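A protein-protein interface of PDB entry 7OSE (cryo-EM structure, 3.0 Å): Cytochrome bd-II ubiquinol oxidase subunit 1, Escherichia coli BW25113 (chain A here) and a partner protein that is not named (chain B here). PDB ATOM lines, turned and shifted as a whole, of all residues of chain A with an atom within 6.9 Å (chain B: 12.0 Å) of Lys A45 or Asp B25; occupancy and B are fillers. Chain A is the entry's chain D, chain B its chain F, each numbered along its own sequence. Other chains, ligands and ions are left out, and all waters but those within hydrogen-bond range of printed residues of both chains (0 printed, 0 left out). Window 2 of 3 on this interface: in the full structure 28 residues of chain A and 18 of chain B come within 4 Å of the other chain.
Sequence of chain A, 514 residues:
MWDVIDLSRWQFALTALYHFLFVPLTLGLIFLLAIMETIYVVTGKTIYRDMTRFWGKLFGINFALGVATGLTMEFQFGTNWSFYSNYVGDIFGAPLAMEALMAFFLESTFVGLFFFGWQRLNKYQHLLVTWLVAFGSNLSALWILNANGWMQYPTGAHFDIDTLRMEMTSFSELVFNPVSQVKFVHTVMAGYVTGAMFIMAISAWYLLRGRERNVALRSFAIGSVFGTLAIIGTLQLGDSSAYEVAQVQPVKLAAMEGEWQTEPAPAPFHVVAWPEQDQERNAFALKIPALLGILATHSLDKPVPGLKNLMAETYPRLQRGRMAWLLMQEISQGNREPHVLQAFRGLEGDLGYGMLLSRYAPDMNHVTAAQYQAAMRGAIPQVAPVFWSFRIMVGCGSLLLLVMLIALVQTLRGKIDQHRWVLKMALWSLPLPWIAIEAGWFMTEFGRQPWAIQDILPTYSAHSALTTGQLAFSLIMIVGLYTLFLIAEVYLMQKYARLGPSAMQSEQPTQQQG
The side-chain carboxylate of Asp B25 lies within salt-bridge range of the guanidinium group of Arg A218 (2.8 Å). NZ of Lys A45 lies close to OD2 of Asp B25 (2.3 Å). The side-chain hydroxyl (OH) of Tyr A48 sits at hydrogen-bond distance from the side-chain carboxylate (OD1) of Asp B25 (2.4 Å).
N of Lys A45 sits close to OG1 of Thr A43. The backbone carbonyl oxygen (O) of Ile A39 is in hydrogen-bond range of the side-chain hydroxyl (OG1) of Thr A43 (2.7 Å). The backbone carbonyl oxygen (O) of Asn A214 lies close to the guanidinium group (NH1) of Arg A218 (3.5 Å).
Among the printed residues, pairs that only touch across the chains: Ile A39 with Thr B18 (3.6 Å), Ile A39 with Leu B21 (3.6 Å), Thr A43 with Val B22 (3.6 Å), Tyr A48 with Leu B21 (3.7 Å), Arg A218 with Leu B21 (3.9 Å) and Arg A218 with Leu B28 (3.7 Å).
Val A41 touches none of the printed residues of chain B. Thr A43 touches one residue of chain B. Gly A44 touches none of the printed residues of chain B. Of chain B, only Asp B25 (2.3 Å) comes within 4 Å of Lys A45. No residue of chain B comes within 4 Å of Thr A46. No residue of chain B comes within 4 Å of Ile A47. Tyr A48 touches just these residues of chain B: Leu B21 (3.7 Å) and Asp B25 (2.4 Å). No residue of chain B comes within 4 Å of Arg A49. Arg A218 touches three residues of chain B. Of the printed residues of chain A, Thr B18 touches Ile A39 (3.6 Å). Of the printed residues of chain A, Leu B21 touches Ile A39 (3.6 Å), Tyr A48 (3.7 Å) and Arg A218 (3.9 Å). Asp B25 touches just these residues of chain A: Lys A45, Tyr A48 and Arg A218.
Printed residues of chain B that touch a printed residue of chain A: Thr B18, Leu B21, Val B22, Asp B25 and Leu B28. Hydrophobic or aromatic side chains of chain B within 4 Å of the printed part of chain A: Leu B21, Val B22 and Leu B28. Along chain B the printed residues that touch a printed residue of chain A span positions 18 to 28.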
ATOM      1  N   MET A  36     -17.675 -36.647  26.269  1.00  0.00           N
ATOM      2  CA  MET A  36     -18.138 -36.210  24.956  1.00  0.00           C
ATOM      3  C   MET A  36     -19.343 -37.023  24.500  1.00  0.00           C
ATOM      4  O   MET A  36     -20.305 -36.470  23.953  1.00  0.00           O
ATOM      5  CB  MET A  36     -16.996 -36.304  23.949  1.00  0.00           C
ATOM      6  CG  MET A  36     -15.827 -35.410  24.305  1.00  0.00           C
ATOM      7  SD  MET A  36     -14.282 -35.885  23.519  1.00  0.00           S
ATOM      8  CE  MET A  36     -13.129 -34.899  24.468  1.00  0.00           C
ATOM      9  N   ILE A  39     -22.397 -35.848  26.459  1.00  0.00           N
ATOM     10  CA  ILE A  39     -22.891 -34.577  25.940  1.00  0.00           C
ATOM     11  C   ILE A  39     -23.638 -34.794  24.632  1.00  0.00           C
ATOM     12  O   ILE A  39     -24.688 -34.186  24.392  1.00  0.00           O
ATOM     13  CB  ILE A  39     -21.735 -33.576  25.773  1.00  0.00           C
ATOM     14  CG1 ILE A  39     -21.084 -33.284  27.124  1.00  0.00           C
ATOM     15  CG2 ILE A  39     -22.239 -32.285  25.163  1.00  0.00           C
ATOM     16  CD1 ILE A  39     -19.761 -32.571  27.012  1.00  0.00           C
ATOM     17  N   TYR A  40     -23.111 -35.663  23.766  1.00  0.00           N
ATOM     18  CA  TYR A  40     -23.799 -35.954  22.512  1.00  0.00           C
ATOM     19  C   TYR A  40     -25.165 -36.580  22.762  1.00  0.00           C
ATOM     20  O   TYR A  40     -26.142 -36.245  22.085  1.00  0.00           O
ATOM     21  CB  TYR A  40     -22.946 -36.874  21.642  1.00  0.00           C
ATOM     22  CG  TYR A  40     -23.745 -37.653  20.623  1.00  0.00           C
ATOM     23  CD1 TYR A  40     -24.245 -37.038  19.486  1.00  0.00           C
ATOM     24  CD2 TYR A  40     -23.999 -39.006  20.802  1.00  0.00           C
ATOM     25  CE1 TYR A  40     -24.978 -37.746  18.555  1.00  0.00           C
ATOM     26  CE2 TYR A  40     -24.729 -39.722  19.876  1.00  0.00           C
ATOM     27  CZ  TYR A  40     -25.215 -39.088  18.755  1.00  0.00           C
ATOM     28  OH  TYR A  40     -25.943 -39.799  17.831  1.00  0.00           O
ATOM     29  N   VAL A  41     -25.250 -37.499  23.723  1.00  0.00           N
ATOM     30  CA  VAL A  41     -26.526 -38.145  24.017  1.00  0.00           C
ATOM     31  C   VAL A  41     -27.518 -37.143  24.594  1.00  0.00           C
ATOM     32  O   VAL A  41     -28.696 -37.129  24.218  1.00  0.00           O
ATOM     33  CB  VAL A  41     -26.314 -39.344  24.958  1.00  0.00           C
ATOM     34  CG1 VAL A  41     -27.648 -39.871  25.453  1.00  0.00           C
ATOM     35  CG2 VAL A  41     -25.547 -40.442  24.247  1.00  0.00           C
ATOM     36  N   VAL A  42     -27.061 -36.283  25.504  1.00  0.00           N
ATOM     37  CA  VAL A  42     -27.971 -35.374  26.197  1.00  0.00           C
ATOM     38  C   VAL A  42     -28.414 -34.241  25.278  1.00  0.00           C
ATOM     39  O   VAL A  42     -29.610 -34.060  25.021  1.00  0.00           O
ATOM     40  CB  VAL A  42     -27.314 -34.833  27.479  1.00  0.00           C
ATOM     41  CG1 VAL A  42     -28.144 -33.707  28.060  1.00  0.00           C
ATOM     42  CG2 VAL A  42     -27.146 -35.947  28.494  1.00  0.00           C
ATOM     43  N   THR A  43     -27.459 -33.453  24.780  1.00  0.00           N
ATOM     44  CA  THR A  43     -27.808 -32.315  23.935  1.00  0.00           C
ATOM     45  C   THR A  43     -28.366 -32.755  22.589  1.00  0.00           C
ATOM     46  O   THR A  43     -29.272 -32.106  22.054  1.00  0.00           O
ATOM     47  CB  THR A  43     -26.589 -31.420  23.723  1.00  0.00           C
ATOM     48  OG1 THR A  43     -25.613 -32.118  22.942  1.00  0.00           O
ATOM     49  CG2 THR A  43     -25.976 -31.034  25.055  1.00  0.00           C
ATOM     50  N   GLY A  44     -27.841 -33.841  22.025  1.00  0.00           N
ATOM     51  CA  GLY A  44     -28.250 -34.301  20.719  1.00  0.00           C
ATOM     52  C   GLY A  44     -27.461 -33.724  19.564  1.00  0.00           C
ATOM     53  O   GLY A  44     -27.661 -34.158  18.422  1.00  0.00           O
ATOM     54  N   LYS A  45     -26.572 -32.769  19.821  1.00  0.00           N
ATOM     55  CA  LYS A  45     -25.779 -32.174  18.756  1.00  0.00           C
ATOM     56  C   LYS A  45     -24.715 -33.151  18.272  1.00  0.00           C
ATOM     57  O   LYS A  45     -24.082 -33.851  19.067  1.00  0.00           O
ATOM     58  CB  LYS A  45     -25.130 -30.880  19.246  1.00  0.00           C
ATOM     59  CG  LYS A  45     -26.122 -29.908  19.858  1.00  0.00           C
ATOM     60  CD  LYS A  45     -25.438 -28.685  20.437  1.00  0.00           C
ATOM     61  CE  LYS A  45     -26.453 -27.756  21.085  1.00  0.00           C
ATOM     62  NZ  LYS A  45     -25.820 -26.539  21.658  1.00  0.00           N
ATOM     63  N   THR A  46     -24.517 -33.192  16.955  1.00  0.00           N
ATOM     64  CA  THR A  46     -23.617 -34.165  16.348  1.00  0.00           C
ATOM     65  C   THR A  46     -22.156 -33.741  16.383  1.00  0.00           C
ATOM     66  O   THR A  46     -21.294 -34.530  15.984  1.00  0.00           O
ATOM     67  CB  THR A  46     -24.030 -34.433  14.900  1.00  0.00           C
ATOM     68  OG1 THR A  46     -24.149 -33.190  14.198  1.00  0.00           O
ATOM     69  CG2 THR A  46     -25.361 -35.164  14.856  1.00  0.00           C
ATOM     70  N   ILE A  47     -21.854 -32.524  16.839  1.00  0.00           N
ATOM     71  CA  ILE A  47     -20.464 -32.083  16.909  1.00  0.00           C
ATOM     72  C   ILE A  47     -19.681 -32.948  17.887  1.00  0.00           C
ATOM     73  O   ILE A  47     -18.542 -33.349  17.615  1.00  0.00           O
ATOM     74  CB  ILE A  47     -20.396 -30.593  17.290  1.00  0.00           C
ATOM     75  CG1 ILE A  47     -21.199 -29.755  16.295  1.00  0.00           C
ATOM     76  CG2 ILE A  47     -18.953 -30.121  17.347  1.00  0.00           C
ATOM     77  CD1 ILE A  47     -21.258 -28.285  16.640  1.00  0.00           C
ATOM     78  N   TYR A  48     -20.282 -33.256  19.037  1.00  0.00           N
ATOM     79  CA  TYR A  48     -19.586 -34.039  20.049  1.00  0.00           C
ATOM     80  C   TYR A  48     -19.337 -35.468  19.588  1.00  0.00           C
ATOM     81  O   TYR A  48     -18.378 -36.100  20.041  1.00  0.00           O
ATOM     82  CB  TYR A  48     -20.374 -34.011  21.356  1.00  0.00           C
ATOM     83  CG  TYR A  48     -20.500 -32.615  21.920  1.00  0.00           C
ATOM     84  CD1 TYR A  48     -19.518 -32.091  22.749  1.00  0.00           C
ATOM     85  CD2 TYR A  48     -21.587 -31.813  21.604  1.00  0.00           C
ATOM     86  CE1 TYR A  48     -19.622 -30.813  23.257  1.00  0.00           C
ATOM     87  CE2 TYR A  48     -21.698 -30.534  22.107  1.00  0.00           C
ATOM     88  CZ  TYR A  48     -20.714 -30.039  22.934  1.00  0.00           C
ATOM     89  OH  TYR A  48     -20.823 -28.764  23.439  1.00  0.00           O
ATOM     90  N   ARG A  49     -20.169 -35.994  18.688  1.00  0.00           N
ATOM     91  CA  ARG A  49     -19.876 -37.300  18.106  1.00  0.00           C
ATOM     92  C   ARG A  49     -18.597 -37.257  17.279  1.00  0.00           C
ATOM     93  O   ARG A  49     -17.755 -38.159  17.370  1.00  0.00           O
ATOM     94  CB  ARG A  49     -21.054 -37.773  17.256  1.00  0.00           C
ATOM     95  CG  ARG A  49     -20.907 -39.191  16.733  1.00  0.00           C
ATOM     96  CD  ARG A  49     -22.099 -39.581  15.883  1.00  0.00           C
ATOM     97  NE  ARG A  49     -22.305 -38.651  14.780  1.00  0.00           N
ATOM     98  CZ  ARG A  49     -23.350 -38.673  13.967  1.00  0.00           C
ATOM     99  NH1 ARG A  49     -24.314 -39.570  14.104  1.00  0.00           N
ATOM    100  NH2 ARG A  49     -23.434 -37.773  12.991  1.00  0.00           N
ATOM    101  N   ASP A  50     -18.427 -36.208  16.473  1.00  0.00           N
ATOM    102  CA  ASP A  50     -17.179 -36.048  15.732  1.00  0.00           C
ATOM    103  C   ASP A  50     -16.004 -35.876  16.682  1.00  0.00           C
ATOM    104  O   ASP A  50     -14.922 -36.434  16.456  1.00  0.00           O
ATOM    105  CB  ASP A  50     -17.283 -34.857  14.783  1.00  0.00           C
ATOM    106  CG  ASP A  50     -18.521 -34.912  13.915  1.00  0.00           C
ATOM    107  OD1 ASP A  50     -19.277 -35.901  14.020  1.00  0.00           O
ATOM    108  OD2 ASP A  50     -18.742 -33.967  13.129  1.00  0.00           O
ATOM    109  N   ASN A 214     -14.576 -25.250  16.166  1.00  0.00           N
ATOM    110  CA  ASN A 214     -15.761 -25.864  16.753  1.00  0.00           C
ATOM    111  C   ASN A 214     -15.382 -27.005  17.690  1.00  0.00           C
ATOM    112  O   ASN A 214     -15.730 -26.987  18.874  1.00  0.00           O
ATOM    113  CB  ASN A 214     -16.701 -26.357  15.648  1.00  0.00           C
ATOM    114  CG  ASN A 214     -17.199 -25.233  14.763  1.00  0.00           C
ATOM    115  OD1 ASN A 214     -17.271 -24.080  15.186  1.00  0.00           O
ATOM    116  ND2 ASN A 214     -17.548 -25.564  13.526  1.00  0.00           N
ATOM    117  N   ARG A 218     -14.845 -26.721  22.286  1.00  0.00           N
ATOM    118  CA  ARG A 218     -15.520 -27.642  23.195  1.00  0.00           C
ATOM    119  C   ARG A 218     -14.522 -28.565  23.882  1.00  0.00           C
ATOM    120  O   ARG A 218     -14.625 -28.815  25.090  1.00  0.00           O
ATOM    121  CB  ARG A 218     -16.570 -28.459  22.441  1.00  0.00           C
ATOM    122  CG  ARG A 218     -17.912 -27.767  22.257  1.00  0.00           C
ATOM    123  CD  ARG A 218     -17.883 -26.786  21.102  1.00  0.00           C
ATOM    124  NE  ARG A 218     -19.215 -26.300  20.760  1.00  0.00           N
ATOM    125  CZ  ARG A 218     -19.465 -25.421  19.800  1.00  0.00           C
ATOM    126  NH1 ARG A 218     -18.494 -24.909  19.062  1.00  0.00           N
ATOM    127  NH2 ARG A 218     -20.721 -25.045  19.576  1.00  0.00           N
ATOM    128  N   LEU B  16     -20.289 -32.545  36.274  1.00  0.00           N
ATOM    129  CA  LEU B  16     -19.971 -31.122  36.256  1.00  0.00           C
ATOM    130  C   LEU B  16     -19.454 -30.687  34.893  1.00  0.00           C
ATOM    131  O   LEU B  16     -19.850 -29.637  34.379  1.00  0.00           O
ATOM    132  CB  LEU B  16     -18.947 -30.794  37.342  1.00  0.00           C
ATOM    133  CG  LEU B  16     -19.473 -30.193  38.644  1.00  0.00           C
ATOM    134  CD1 LEU B  16     -20.137 -28.854  38.376  1.00  0.00           C
ATOM    135  CD2 LEU B  16     -20.437 -31.141  39.329  1.00  0.00           C
ATOM    136  N   SER B  17     -18.563 -31.482  34.293  1.00  0.00           N
ATOM    137  CA  SER B  17     -18.072 -31.147  32.961  1.00  0.00           C
ATOM    138  C   SER B  17     -19.205 -31.154  31.945  1.00  0.00           C
ATOM    139  O   SER B  17     -19.297 -30.254  31.099  1.00  0.00           O
ATOM    140  CB  SER B  17     -16.970 -32.120  32.549  1.00  0.00           C
ATOM    141  OG  SER B  17     -15.891 -32.081  33.465  1.00  0.00           O
ATOM    142  N   THR B  18     -20.086 -32.154  32.023  1.00  0.00           N
ATOM    143  CA  THR B  18     -21.212 -32.217  31.099  1.00  0.00           C
ATOM    144  C   THR B  18     -22.114 -30.997  31.247  1.00  0.00           C
ATOM    145  O   THR B  18     -22.530 -30.394  30.253  1.00  0.00           O
ATOM    146  CB  THR B  18     -22.007 -33.503  31.327  1.00  0.00           C
ATOM    147  OG1 THR B  18     -21.110 -34.616  31.391  1.00  0.00           O
ATOM    148  CG2 THR B  18     -22.986 -33.724  30.189  1.00  0.00           C
ATOM    149  N   LEU B  19     -22.422 -30.614  32.489  1.00  0.00           N
ATOM    150  CA  LEU B  19     -23.284 -29.459  32.721  1.00  0.00           C
ATOM    151  C   LEU B  19     -22.637 -28.171  32.234  1.00  0.00           C
ATOM    152  O   LEU B  19     -23.303 -27.324  31.626  1.00  0.00           O
ATOM    153  CB  LEU B  19     -23.629 -29.349  34.204  1.00  0.00           C
ATOM    154  CG  LEU B  19     -24.781 -30.224  34.684  1.00  0.00           C
ATOM    155  CD1 LEU B  19     -25.064 -29.972  36.154  1.00  0.00           C
ATOM    156  CD2 LEU B  19     -26.010 -29.949  33.843  1.00  0.00           C
ATOM    157  N   VAL B  20     -21.342 -27.998  32.502  1.00  0.00           N
ATOM    158  CA  VAL B  20     -20.654 -26.790  32.062  1.00  0.00           C
ATOM    159  C   VAL B  20     -20.658 -26.703  30.544  1.00  0.00           C
ATOM    160  O   VAL B  20     -20.862 -25.627  29.971  1.00  0.00           O
ATOM    161  CB  VAL B  20     -19.226 -26.746  32.634  1.00  0.00           C
ATOM    162  CG1 VAL B  20     -18.403 -25.685  31.929  1.00  0.00           C
ATOM    163  CG2 VAL B  20     -19.270 -26.472  34.125  1.00  0.00           C
ATOM    164  N   LEU B  21     -20.449 -27.832  29.865  1.00  0.00           N
ATOM    165  CA  LEU B  21     -20.462 -27.807  28.407  1.00  0.00           C
ATOM    166  C   LEU B  21     -21.861 -27.552  27.858  1.00  0.00           C
ATOM    167  O   LEU B  21     -22.016 -26.867  26.842  1.00  0.00           O
ATOM    168  CB  LEU B  21     -19.892 -29.105  27.850  1.00  0.00           C
ATOM    169  CG  LEU B  21     -18.450 -28.967  27.372  1.00  0.00           C
ATOM    170  CD1 LEU B  21     -18.394 -28.125  26.111  1.00  0.00           C
ATOM    171  CD2 LEU B  21     -17.577 -28.357  28.456  1.00  0.00           C
ATOM    172  N   VAL B  22     -22.892 -28.100  28.507  1.00  0.00           N
ATOM    173  CA  VAL B  22     -24.257 -27.837  28.064  1.00  0.00           C
ATOM    174  C   VAL B  22     -24.583 -26.356  28.202  1.00  0.00           C
ATOM    175  O   VAL B  22     -25.183 -25.749  27.307  1.00  0.00           O
ATOM    176  CB  VAL B  22     -25.258 -28.714  28.840  1.00  0.00           C
ATOM    177  CG1 VAL B  22     -26.681 -28.275  28.549  1.00  0.00           C
ATOM    178  CG2 VAL B  22     -25.080 -30.171  28.470  1.00  0.00           C
ATOM    179  N   TRP B  23     -24.191 -25.750  29.325  1.00  0.00           N
ATOM    180  CA  TRP B  23     -24.449 -24.327  29.521  1.00  0.00           C
ATOM    181  C   TRP B  23     -23.640 -23.470  28.555  1.00  0.00           C
ATOM    182  O   TRP B  23     -24.146 -22.471  28.030  1.00  0.00           O
ATOM    183  CB  TRP B  23     -24.141 -23.933  30.965  1.00  0.00           C
ATOM    184  CG  TRP B  23     -24.040 -22.454  31.169  1.00  0.00           C
ATOM    185  CD1 TRP B  23     -25.070 -21.568  31.265  1.00  0.00           C
ATOM    186  CD2 TRP B  23     -22.837 -21.688  31.303  1.00  0.00           C
ATOM    187  NE1 TRP B  23     -24.586 -20.298  31.449  1.00  0.00           N
ATOM    188  CE2 TRP B  23     -23.216 -20.344  31.476  1.00  0.00           C
ATOM    189  CE3 TRP B  23     -21.477 -22.008  31.293  1.00  0.00           C
ATOM    190  CZ2 TRP B  23     -22.286 -19.320  31.639  1.00  0.00           C
ATOM    191  CZ3 TRP B  23     -20.556 -20.991  31.453  1.00  0.00           C
ATOM    192  CH2 TRP B  23     -20.964 -19.664  31.624  1.00  0.00           C
ATOM    193  N   LEU B  24     -22.387 -23.843  28.303  1.00  0.00           N
ATOM    194  CA  LEU B  24     -21.464 -22.998  27.558  1.00  0.00           C
ATOM    195  C   LEU B  24     -21.553 -23.181  26.050  1.00  0.00           C
ATOM    196  O   LEU B  24     -21.041 -22.332  25.311  1.00  0.00           O
ATOM    197  CB  LEU B  24     -20.029 -23.273  28.021  1.00  0.00           C
ATOM    198  CG  LEU B  24     -18.927 -22.294  27.615  1.00  0.00           C
ATOM    199  CD1 LEU B  24     -19.268 -20.885  28.060  1.00  0.00           C
ATOM    200  CD2 LEU B  24     -17.598 -22.734  28.199  1.00  0.00           C
ATOM    201  N   ASP B  25     -22.188 -24.250  25.572  1.00  0.00           N
ATOM    202  CA  ASP B  25     -22.220 -24.502  24.132  1.00  0.00           C
ATOM    203  C   ASP B  25     -22.900 -23.387  23.346  1.00  0.00           C
ATOM    204  O   ASP B  25     -22.327 -22.943  22.337  1.00  0.00           O
ATOM    205  CB  ASP B  25     -22.874 -25.861  23.858  1.00  0.00           C
ATOM    206  CG  ASP B  25     -22.680 -26.321  22.427  1.00  0.00           C
ATOM    207  OD1 ASP B  25     -21.612 -26.893  22.125  1.00  0.00           O
ATOM    208  OD2 ASP B  25     -23.590 -26.105  21.600  1.00  0.00           O
ATOM    209  N   PRO B  26     -24.090 -22.897  23.717  1.00  0.00           N
ATOM    210  CA  PRO B  26     -24.666 -21.771  22.962  1.00  0.00           C
ATOM    211  C   PRO B  26     -23.825 -20.510  23.019  1.00  0.00           C
ATOM    212  O   PRO B  26     -23.828 -19.731  22.058  1.00  0.00           O
ATOM    213  CB  PRO B  26     -26.035 -21.567  23.627  1.00  0.00           C
ATOM    214  CG  PRO B  26     -26.337 -22.862  24.286  1.00  0.00           C
ATOM    215  CD  PRO B  26     -25.017 -23.368  24.761  1.00  0.00           C
ATOM    216  N   ARG B  27     -23.104 -20.282  24.118  1.00  0.00           N
ATOM    217  CA  ARG B  27     -22.329 -19.059  24.280  1.00  0.00           C
ATOM    218  C   ARG B  27     -21.062 -19.038  23.437  1.00  0.00           C
ATOM    219  O   ARG B  27     -20.430 -17.983  23.331  1.00  0.00           O
ATOM    220  CB  ARG B  27     -21.974 -18.863  25.755  1.00  0.00           C
ATOM    221  CG  ARG B  27     -23.183 -18.794  26.674  1.00  0.00           C
ATOM    222  CD  ARG B  27     -22.782 -18.963  28.129  1.00  0.00           C
ATOM    223  NE  ARG B  27     -21.856 -17.928  28.570  1.00  0.00           N
ATOM    224  CZ  ARG B  27     -22.222 -16.786  29.135  1.00  0.00           C
ATOM    225  NH1 ARG B  27     -23.497 -16.498  29.344  1.00  0.00           N
ATOM    226  NH2 ARG B  27     -21.289 -15.912  29.498  1.00  0.00           N
ATOM    227  N   LEU B  28     -20.674 -20.162  22.844  1.00  0.00           N
ATOM    228  CA  LEU B  28     -19.466 -20.218  22.030  1.00  0.00           C
ATOM    229  C   LEU B  28     -19.732 -19.718  20.615  1.00  0.00           C
ATOM    230  O   LEU B  28     -18.800 -19.415  19.870  1.00  0.00           O
ATOM    231  CB  LEU B  28     -18.915 -21.645  21.989  1.00  0.00           C
ATOM    232  CG  LEU B  28     -18.438 -22.217  23.325  1.00  0.00           C
ATOM    233  CD1 LEU B  28     -18.063 -23.680  23.180  1.00  0.00           C
ATOM    234  CD2 LEU B  28     -17.266 -21.413  23.861  1.00  0.00           C
